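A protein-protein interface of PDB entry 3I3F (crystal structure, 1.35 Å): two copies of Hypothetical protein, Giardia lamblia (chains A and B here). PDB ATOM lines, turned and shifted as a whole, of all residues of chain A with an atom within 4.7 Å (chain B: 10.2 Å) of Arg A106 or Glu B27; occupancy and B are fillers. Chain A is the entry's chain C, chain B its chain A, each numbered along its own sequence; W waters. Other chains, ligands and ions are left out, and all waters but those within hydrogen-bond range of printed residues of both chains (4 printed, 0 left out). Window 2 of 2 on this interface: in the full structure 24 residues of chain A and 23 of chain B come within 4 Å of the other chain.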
ATOM      1  N   ASN A 102     -31.478  -2.817 -18.458  1.00  0.00           N
ATOM      2  CA  ASN A 102     -31.144  -1.465 -18.903  1.00  0.00           C
ATOM      3  C   ASN A 102     -30.444  -0.632 -17.826  1.00  0.00           C
ATOM      4  O   ASN A 102     -29.594   0.194 -18.150  1.00  0.00           O
ATOM      5  CB  ASN A 102     -32.377  -0.760 -19.476  1.00  0.00           C
ATOM      6  CG  ASN A 102     -32.755  -1.294 -20.848  1.00  0.00           C
ATOM      7  OD1 ASN A 102     -31.898  -1.439 -21.724  1.00  0.00           O
ATOM      8  ND2 ASN A 102     -34.031  -1.605 -21.038  1.00  0.00           N
ATOM      9  N   GLU A 103     -30.779  -0.861 -16.554  1.00  0.00           N
ATOM     10  CA  GLU A 103     -30.065  -0.213 -15.459  1.00  0.00           C
ATOM     11  C   GLU A 103     -28.602  -0.657 -15.453  1.00  0.00           C
ATOM     12  O   GLU A 103     -27.701   0.171 -15.334  1.00  0.00           O
ATOM     13  CB  GLU A 103     -30.723  -0.527 -14.113  1.00  0.00           C
ATOM     14  CG  GLU A 103     -30.229   0.348 -12.972  1.00  0.00           C
ATOM     15  CD  GLU A 103     -30.929   0.052 -11.664  1.00  0.00           C
ATOM     16  OE1 GLU A 103     -31.695  -0.933 -11.607  1.00  0.00           O
ATOM     17  OE2 GLU A 103     -30.706   0.800 -10.688  1.00  0.00           O
ATOM     18  N   LEU A 104     -28.374  -1.959 -15.594  1.00  0.00           N
ATOM     19  CA  LEU A 104     -27.016  -2.500 -15.645  1.00  0.00           C
ATOM     20  C   LEU A 104     -26.278  -2.019 -16.891  1.00  0.00           C
ATOM     21  O   LEU A 104     -25.079  -1.752 -16.843  1.00  0.00           O
ATOM     22  CB  LEU A 104     -27.042  -4.030 -15.617  1.00  0.00           C
ATOM     23  CG  LEU A 104     -27.571  -4.664 -14.328  1.00  0.00           C
ATOM     24  CD1 LEU A 104     -27.695  -6.167 -14.497  1.00  0.00           C
ATOM     25  CD2 LEU A 104     -26.685  -4.330 -13.138  1.00  0.00           C
ATOM     26  N   TYR A 105     -27.001  -1.912 -18.004  1.00  0.00           N
ATOM     27  CA  TYR A 105     -26.438  -1.405 -19.254  1.00  0.00           C
ATOM     28  C   TYR A 105     -25.920   0.023 -19.082  1.00  0.00           C
ATOM     29  O   TYR A 105     -24.837   0.361 -19.564  1.00  0.00           O
ATOM     30  CB  TYR A 105     -27.491  -1.452 -20.360  1.00  0.00           C
ATOM     31  CG  TYR A 105     -26.963  -1.099 -21.731  1.00  0.00           C
ATOM     32  CD1 TYR A 105     -26.411  -2.072 -22.555  1.00  0.00           C
ATOM     33  CD2 TYR A 105     -27.017   0.210 -22.202  1.00  0.00           C
ATOM     34  CE1 TYR A 105     -25.926  -1.753 -23.814  1.00  0.00           C
ATOM     35  CE2 TYR A 105     -26.538   0.538 -23.460  1.00  0.00           C
ATOM     36  CZ  TYR A 105     -25.990  -0.451 -24.260  1.00  0.00           C
ATOM     37  OH  TYR A 105     -25.509  -0.150 -25.512  1.00  0.00           O
ATOM     38  N   ARG A 106     -26.692   0.851 -18.383  1.00  0.00           N
ATOM     39  CA  ARG A 106     -26.296   2.234 -18.111  1.00  0.00           C
ATOM     40  C   ARG A 106     -25.123   2.338 -17.129  1.00  0.00           C
ATOM     41  O   ARG A 106     -24.458   3.367 -17.082  1.00  0.00           O
ATOM     42  CB  ARG A 106     -27.491   3.052 -17.609  1.00  0.00           C
ATOM     43  CG  ARG A 106     -28.536   3.336 -18.685  1.00  0.00           C
ATOM     44  CD  ARG A 106     -29.584   4.332 -18.202  1.00  0.00           C
ATOM     45  NE  ARG A 106     -30.424   3.797 -17.130  1.00  0.00           N
ATOM     46  CZ  ARG A 106     -31.536   3.079 -17.303  1.00  0.00           C
ATOM     47  NH1 ARG A 106     -31.974   2.772 -18.520  1.00  0.00           N
ATOM     48  NH2 ARG A 106     -32.216   2.651 -16.242  1.00  0.00           N
ATOM     49  N   GLU A 107     -24.883   1.287 -16.345  1.00  0.00           N
ATOM     50  CA  GLU A 107     -23.687   1.210 -15.494  1.00  0.00           C
ATOM     51  C   GLU A 107     -22.437   0.823 -16.291  1.00  0.00           C
ATOM     52  O   GLU A 107     -21.322   1.159 -15.897  1.00  0.00           O
ATOM     53  CB  GLU A 107     -23.907   0.228 -14.336  1.00  0.00           C
ATOM     54  CG  GLU A 107     -24.954   0.709 -13.340  1.00  0.00           C
ATOM     55  CD  GLU A 107     -25.302  -0.309 -12.266  1.00  0.00           C
ATOM     56  OE1 GLU A 107     -24.778  -1.441 -12.303  1.00  0.00           O
ATOM     57  OE2 GLU A 107     -26.108   0.035 -11.375  1.00  0.00           O
ATOM     58  N   VAL A 108     -22.620   0.114 -17.403  1.00  0.00           N
ATOM     59  CA  VAL A 108     -21.513  -0.206 -18.308  1.00  0.00           C
ATOM     60  C   VAL A 108     -21.187   1.004 -19.185  1.00  0.00           C
ATOM     61  O   VAL A 108     -20.026   1.397 -19.318  1.00  0.00           O
ATOM     62  CB  VAL A 108     -21.852  -1.414 -19.209  1.00  0.00           C
ATOM     63  CG1 VAL A 108     -20.718  -1.693 -20.189  1.00  0.00           C
ATOM     64  CG2 VAL A 108     -22.140  -2.647 -18.363  1.00  0.00           C
ATOM     65  N   PHE A 109     -22.227   1.585 -19.779  1.00  0.00           N
ATOM     66  CA  PHE A 109     -22.096   2.768 -20.624  1.00  0.00           C
ATOM     67  C   PHE A 109     -22.638   3.969 -19.849  1.00  0.00           C
ATOM     68  O   PHE A 109     -23.766   4.411 -20.070  1.00  0.00           O
ATOM     69  CB  PHE A 109     -22.846   2.542 -21.938  1.00  0.00           C
ATOM     70  CG  PHE A 109     -22.340   1.360 -22.717  1.00  0.00           C
ATOM     71  CD1 PHE A 109     -21.191   1.471 -23.484  1.00  0.00           C
ATOM     72  CD2 PHE A 109     -22.992   0.136 -22.664  1.00  0.00           C
ATOM     73  CE1 PHE A 109     -20.702   0.387 -24.200  1.00  0.00           C
ATOM     74  CE2 PHE A 109     -22.510  -0.956 -23.380  1.00  0.00           C
ATOM     75  CZ  PHE A 109     -21.362  -0.827 -24.146  1.00  0.00           C
ATOM     76  N   CYS A 110     -21.805   4.487 -18.946  1.00  0.00           N
ATOM     77  CA  CYS A 110     -22.263   5.499 -17.994  1.00  0.00           C
ATOM     78  C   CYS A 110     -22.181   6.934 -18.509  1.00  0.00           C
ATOM     79  O   CYS A 110     -22.716   7.840 -17.874  1.00  0.00           O
ATOM     80  CB  CYS A 110     -21.500   5.365 -16.680  1.00  0.00           C
ATOM     81  SG  CYS A 110     -19.743   5.222 -16.912  1.00  0.00           S
ATOM     82  N   ARG A 115     -23.015   6.812 -25.727  1.00  0.00           N
ATOM     83  CA  ARG A 115     -23.581   5.466 -25.788  1.00  0.00           C
ATOM     84  C   ARG A 115     -23.651   4.991 -27.233  1.00  0.00           C
ATOM     85  O   ARG A 115     -24.005   5.762 -28.127  1.00  0.00           O
ATOM     86  CB  ARG A 115     -24.960   5.416 -25.130  1.00  0.00           C
ATOM     87  CG  ARG A 115     -24.859   5.428 -23.628  1.00  0.00           C
ATOM     88  CD  ARG A 115     -26.189   5.410 -22.915  1.00  0.00           C
ATOM     89  NE  ARG A 115     -25.920   5.408 -21.479  1.00  0.00           N
ATOM     90  CZ  ARG A 115     -26.662   5.996 -20.542  1.00  0.00           C
ATOM     91  NH1 ARG A 115     -26.267   5.926 -19.279  1.00  0.00           N
ATOM     92  NH2 ARG A 115     -27.784   6.643 -20.844  1.00  0.00           N
ATOM     93  N   VAL B  19     -26.632  13.516 -32.379  1.00  0.00           N
ATOM     94  CA  VAL B  19     -28.073  13.490 -32.169  1.00  0.00           C
ATOM     95  C   VAL B  19     -28.717  14.540 -33.064  1.00  0.00           C
ATOM     96  O   VAL B  19     -28.476  15.738 -32.901  1.00  0.00           O
ATOM     97  CB  VAL B  19     -28.454  13.768 -30.699  1.00  0.00           C
ATOM     98  CG1 VAL B  19     -29.971  13.711 -30.521  1.00  0.00           C
ATOM     99  CG2 VAL B  19     -27.774  12.773 -29.775  1.00  0.00           C
ATOM    100  N   VAL B  23     -35.167  14.364 -34.603  1.00  0.00           N
ATOM    101  CA  VAL B  23     -35.506  12.947 -34.479  1.00  0.00           C
ATOM    102  C   VAL B  23     -35.450  12.523 -33.013  1.00  0.00           C
ATOM    103  O   VAL B  23     -34.530  12.901 -32.282  1.00  0.00           O
ATOM    104  CB  VAL B  23     -34.564  12.060 -35.326  1.00  0.00           C
ATOM    105  CG1 VAL B  23     -34.915  10.582 -35.165  1.00  0.00           C
ATOM    106  CG2 VAL B  23     -34.629  12.469 -36.796  1.00  0.00           C
ATOM    107  N   VAL B  24     -36.441  11.741 -32.592  1.00  0.00           N
ATOM    108  CA  VAL B  24     -36.518  11.246 -31.220  1.00  0.00           C
ATOM    109  C   VAL B  24     -35.218  10.553 -30.795  1.00  0.00           C
ATOM    110  O   VAL B  24     -34.595   9.828 -31.577  1.00  0.00           O
ATOM    111  CB  VAL B  24     -37.723  10.284 -31.030  1.00  0.00           C
ATOM    112  CG1 VAL B  24     -37.556   9.015 -31.863  1.00  0.00           C
ATOM    113  CG2 VAL B  24     -37.918   9.943 -29.561  1.00  0.00           C
ATOM    114  N   LYS B  25     -34.818  10.804 -29.552  1.00  0.00           N
ATOM    115  CA  LYS B  25     -33.598  10.254 -28.975  1.00  0.00           C
ATOM    116  C   LYS B  25     -33.986   9.438 -27.745  1.00  0.00           C
ATOM    117  O   LYS B  25     -34.718   9.926 -26.884  1.00  0.00           O
ATOM    118  CB  LYS B  25     -32.650  11.399 -28.595  1.00  0.00           C
ATOM    119  CG  LYS B  25     -31.390  10.987 -27.837  1.00  0.00           C
ATOM    120  CD  LYS B  25     -30.483  10.112 -28.679  1.00  0.00           C
ATOM    121  CE  LYS B  25     -29.175   9.807 -27.964  1.00  0.00           C
ATOM    122  NZ  LYS B  25     -29.365   8.938 -26.770  1.00  0.00           N
ATOM    123  N   PHE B  26     -33.508   8.197 -27.677  1.00  0.00           N
ATOM    124  CA  PHE B  26     -33.804   7.308 -26.553  1.00  0.00           C
ATOM    125  C   PHE B  26     -32.604   7.232 -25.613  1.00  0.00           C
ATOM    126  O   PHE B  26     -31.461   7.148 -26.064  1.00  0.00           O
ATOM    127  CB  PHE B  26     -34.185   5.914 -27.059  1.00  0.00           C
ATOM    128  CG  PHE B  26     -35.293   5.923 -28.077  1.00  0.00           C
ATOM    129  CD1 PHE B  26     -36.583   6.279 -27.712  1.00  0.00           C
ATOM    130  CD2 PHE B  26     -35.044   5.584 -29.401  1.00  0.00           C
ATOM    131  CE1 PHE B  26     -37.611   6.296 -28.652  1.00  0.00           C
ATOM    132  CE2 PHE B  26     -36.063   5.598 -30.346  1.00  0.00           C
ATOM    133  CZ  PHE B  26     -37.347   5.955 -29.970  1.00  0.00           C
ATOM    134  N   GLU B  27     -32.879   7.252 -24.308  1.00  0.00           N
ATOM    135  CA  GLU B  27     -31.843   7.319 -23.268  1.00  0.00           C
ATOM    136  C   GLU B  27     -30.721   6.298 -23.434  1.00  0.00           C
ATOM    137  O   GLU B  27     -29.546   6.635 -23.286  1.00  0.00           O
ATOM    138  CB  GLU B  27     -32.470   7.131 -21.878  1.00  0.00           C
ATOM    139  CG  GLU B  27     -31.449   7.169 -20.733  1.00  0.00           C
ATOM    140  CD  GLU B  27     -32.070   7.035 -19.353  1.00  0.00           C
ATOM    141  OE1 GLU B  27     -33.179   6.476 -19.235  1.00  0.00           O
ATOM    142  OE2 GLU B  27     -31.430   7.482 -18.379  1.00  0.00           O
ATOM    143  N   ASN B  28     -31.089   5.053 -23.721  1.00  0.00           N
ATOM    144  CA  ASN B  28     -30.122   3.952 -23.766  1.00  0.00           C
ATOM    145  C   ASN B  28     -29.446   3.774 -25.122  1.00  0.00           C
ATOM    146  O   ASN B  28     -28.554   2.936 -25.257  1.00  0.00           O
ATOM    147  CB  ASN B  28     -30.807   2.632 -23.398  1.00  0.00           C
ATOM    148  CG  ASN B  28     -31.467   2.669 -22.033  1.00  0.00           C
ATOM    149  OD1 ASN B  28     -30.938   3.254 -21.086  1.00  0.00           O
ATOM    150  ND2 ASN B  28     -32.627   2.031 -21.923  1.00  0.00           N
ATOM    151  N   VAL B  29     -29.861   4.559 -26.114  1.00  0.00           N
ATOM    152  CA  VAL B  29     -29.573   4.261 -27.511  1.00  0.00           C
ATOM    153  C   VAL B  29     -28.839   5.396 -28.217  1.00  0.00           C
ATOM    154  O   VAL B  29     -29.374   6.496 -28.368  1.00  0.00           O
ATOM    155  CB  VAL B  29     -30.887   3.976 -28.274  1.00  0.00           C
ATOM    156  CG1 VAL B  29     -30.603   3.530 -29.707  1.00  0.00           C
ATOM    157  CG2 VAL B  29     -31.714   2.933 -27.538  1.00  0.00           C
ATOM    158  N   GLY B  30     -27.611   5.124 -28.654  1.00  0.00           N
ATOM    159  CA  GLY B  30     -26.909   6.037 -29.545  1.00  0.00           C
ATOM    160  C   GLY B  30     -27.714   6.154 -30.824  1.00  0.00           C
ATOM    161  O   GLY B  30     -28.071   5.146 -31.433  1.00  0.00           O
ATOM    162  N   GLN B  31     -28.028   7.381 -31.215  1.00  0.00           N
ATOM    163  CA  GLN B  31     -28.871   7.614 -32.381  1.00  0.00           C
ATOM    164  C   GLN B  31     -28.064   7.478 -33.672  1.00  0.00           C
ATOM    165  O   GLN B  31     -28.500   6.832 -34.627  1.00  0.00           O
ATOM    166  CB  GLN B  31     -29.493   9.008 -32.292  1.00  0.00           C
ATOM    167  CG  GLN B  31     -30.677   9.235 -33.210  1.00  0.00           C
ATOM    168  CD  GLN B  31     -31.001  10.703 -33.347  1.00  0.00           C
ATOM    169  OE1 GLN B  31     -30.212  11.461 -33.907  1.00  0.00           O
ATOM    170  NE2 GLN B  31     -32.154  11.118 -32.823  1.00  0.00           N
ATOM    171  N   GLY B  43     -31.362   1.751 -33.343  1.00  0.00           N
ATOM    172  CA  GLY B  43     -32.669   1.285 -33.797  1.00  0.00           C
ATOM    173  C   GLY B  43     -33.616   2.437 -34.072  1.00  0.00           C
ATOM    174  O   GLY B  43     -33.682   3.391 -33.292  1.00  0.00           O
ATOM    175  N   GLN B 126     -40.586  -4.199 -28.574  1.00  0.00           N
ATOM    176  CA  GLN B 126     -41.057  -3.497 -27.379  1.00  0.00           C
ATOM    177  C   GLN B 126     -42.494  -3.006 -27.572  1.00  0.00           C
ATOM    178  O   GLN B 126     -42.978  -2.901 -28.702  1.00  0.00           O
ATOM    179  CB  GLN B 126     -40.113  -2.343 -27.022  1.00  0.00           C
ATOM    180  CG  GLN B 126     -38.746  -2.819 -26.525  1.00  0.00           C
ATOM    181  CD  GLN B 126     -37.718  -1.708 -26.419  1.00  0.00           C
ATOM    182  OE1 GLN B 126     -38.059  -0.525 -26.367  1.00  0.00           O
ATOM    183  NE2 GLN B 126     -36.444  -2.087 -26.377  1.00  0.00           N
HETATM  184  O   HOH W   1     -28.948   8.349 -18.894  1.00  0.00           O
HETATM  185  O   HOH W   2     -34.543   2.261 -19.572  1.00  0.00           O
HETATM  186  O   HOH W   3     -26.127   2.298 -26.246  1.00  0.00           O
HETATM  187  O   HOH W   4     -34.567  -2.914 -23.647  1.00  0.00           O
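The side-chain carboxylate (OE1) of Glu B27 lies within salt-bridge range of the guanidinium group (NH1) of Arg A106 (3.96 Å).
The backbone carbonyl oxygen of Glu B27 sits at hydrogen-bond distance from the guanidinium group of Arg A115 (3.0 Å).
The side-chain amide oxygen of Asn B28 lies within hydrogen-bond range of the guanidinium group of Arg A106 (2.8 Å).
O of Phe A109 lies within hydrogen-bond range of NE of Arg A115, 2.8 Å away.
Asn B28 touches Asn A102.
Tyr A105 touches Asn B28.
Gly B30 touches Arg A115 (CA to O, 3.2 Å).
Of chain B, only Asn B28 (3.5 Å) comes within 4 Å of Asn A102.
Of the printed residues of chain B, Tyr A105 touches Asn B28.
Of chain B, only Glu B27 (3.7 Å) and Asn B28 (2.8 Å) come within 4 Å of Arg A106.
Cys A110 touches none of the printed residues of chain B.
Printed residues of chain B within 4 Å of Arg A115: Glu B27 (3.0 Å) and Gly B30 (3.2 Å).
Glu B27 touches just these residues of chain A: Arg A106 (3.7 Å) and Arg A115 (3.0 Å).
Of the printed residues of chain A, Asn B28 touches Asn A102, Tyr A105 and Arg A106.
Val B29 touches none of the printed residues of chain A.
Of the printed residues of chain A, Gly B30 touches Arg A115.
The nearest residue of chain B that does not touch Arg A106 is Val B29 (7.6 Å).
The nearest printed residue of chain A that does not touch Glu B27 is Tyr A105 (6.8 Å).
The nearest printed residue of chain A that does not touch Gly B30 is Tyr A105 (6.5 Å).
Among the printed residues, 6 pairs touch across the chains.
No position is printed for both chains.
Water W3 lies within hydrogen-bond range of the side-chain hydroxyl (OH) of Tyr A105 and the backbone carbonyl oxygen (O) of Asn B28.
Water W1 lies within hydrogen-bond range of the side-chain carboxylate (OE2) of Glu B27 and the guanidinium group (NH2) of Arg A115.
Water W2 lies within hydrogen-bond range of the guanidinium group of Arg A106 (2.8 Å) and the side-chain amide nitrogen of Asn B28 (3.0 Å).
Water W4 lies within hydrogen-bond range of ND2 of Asn A102 and NE2 of Gln B126.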
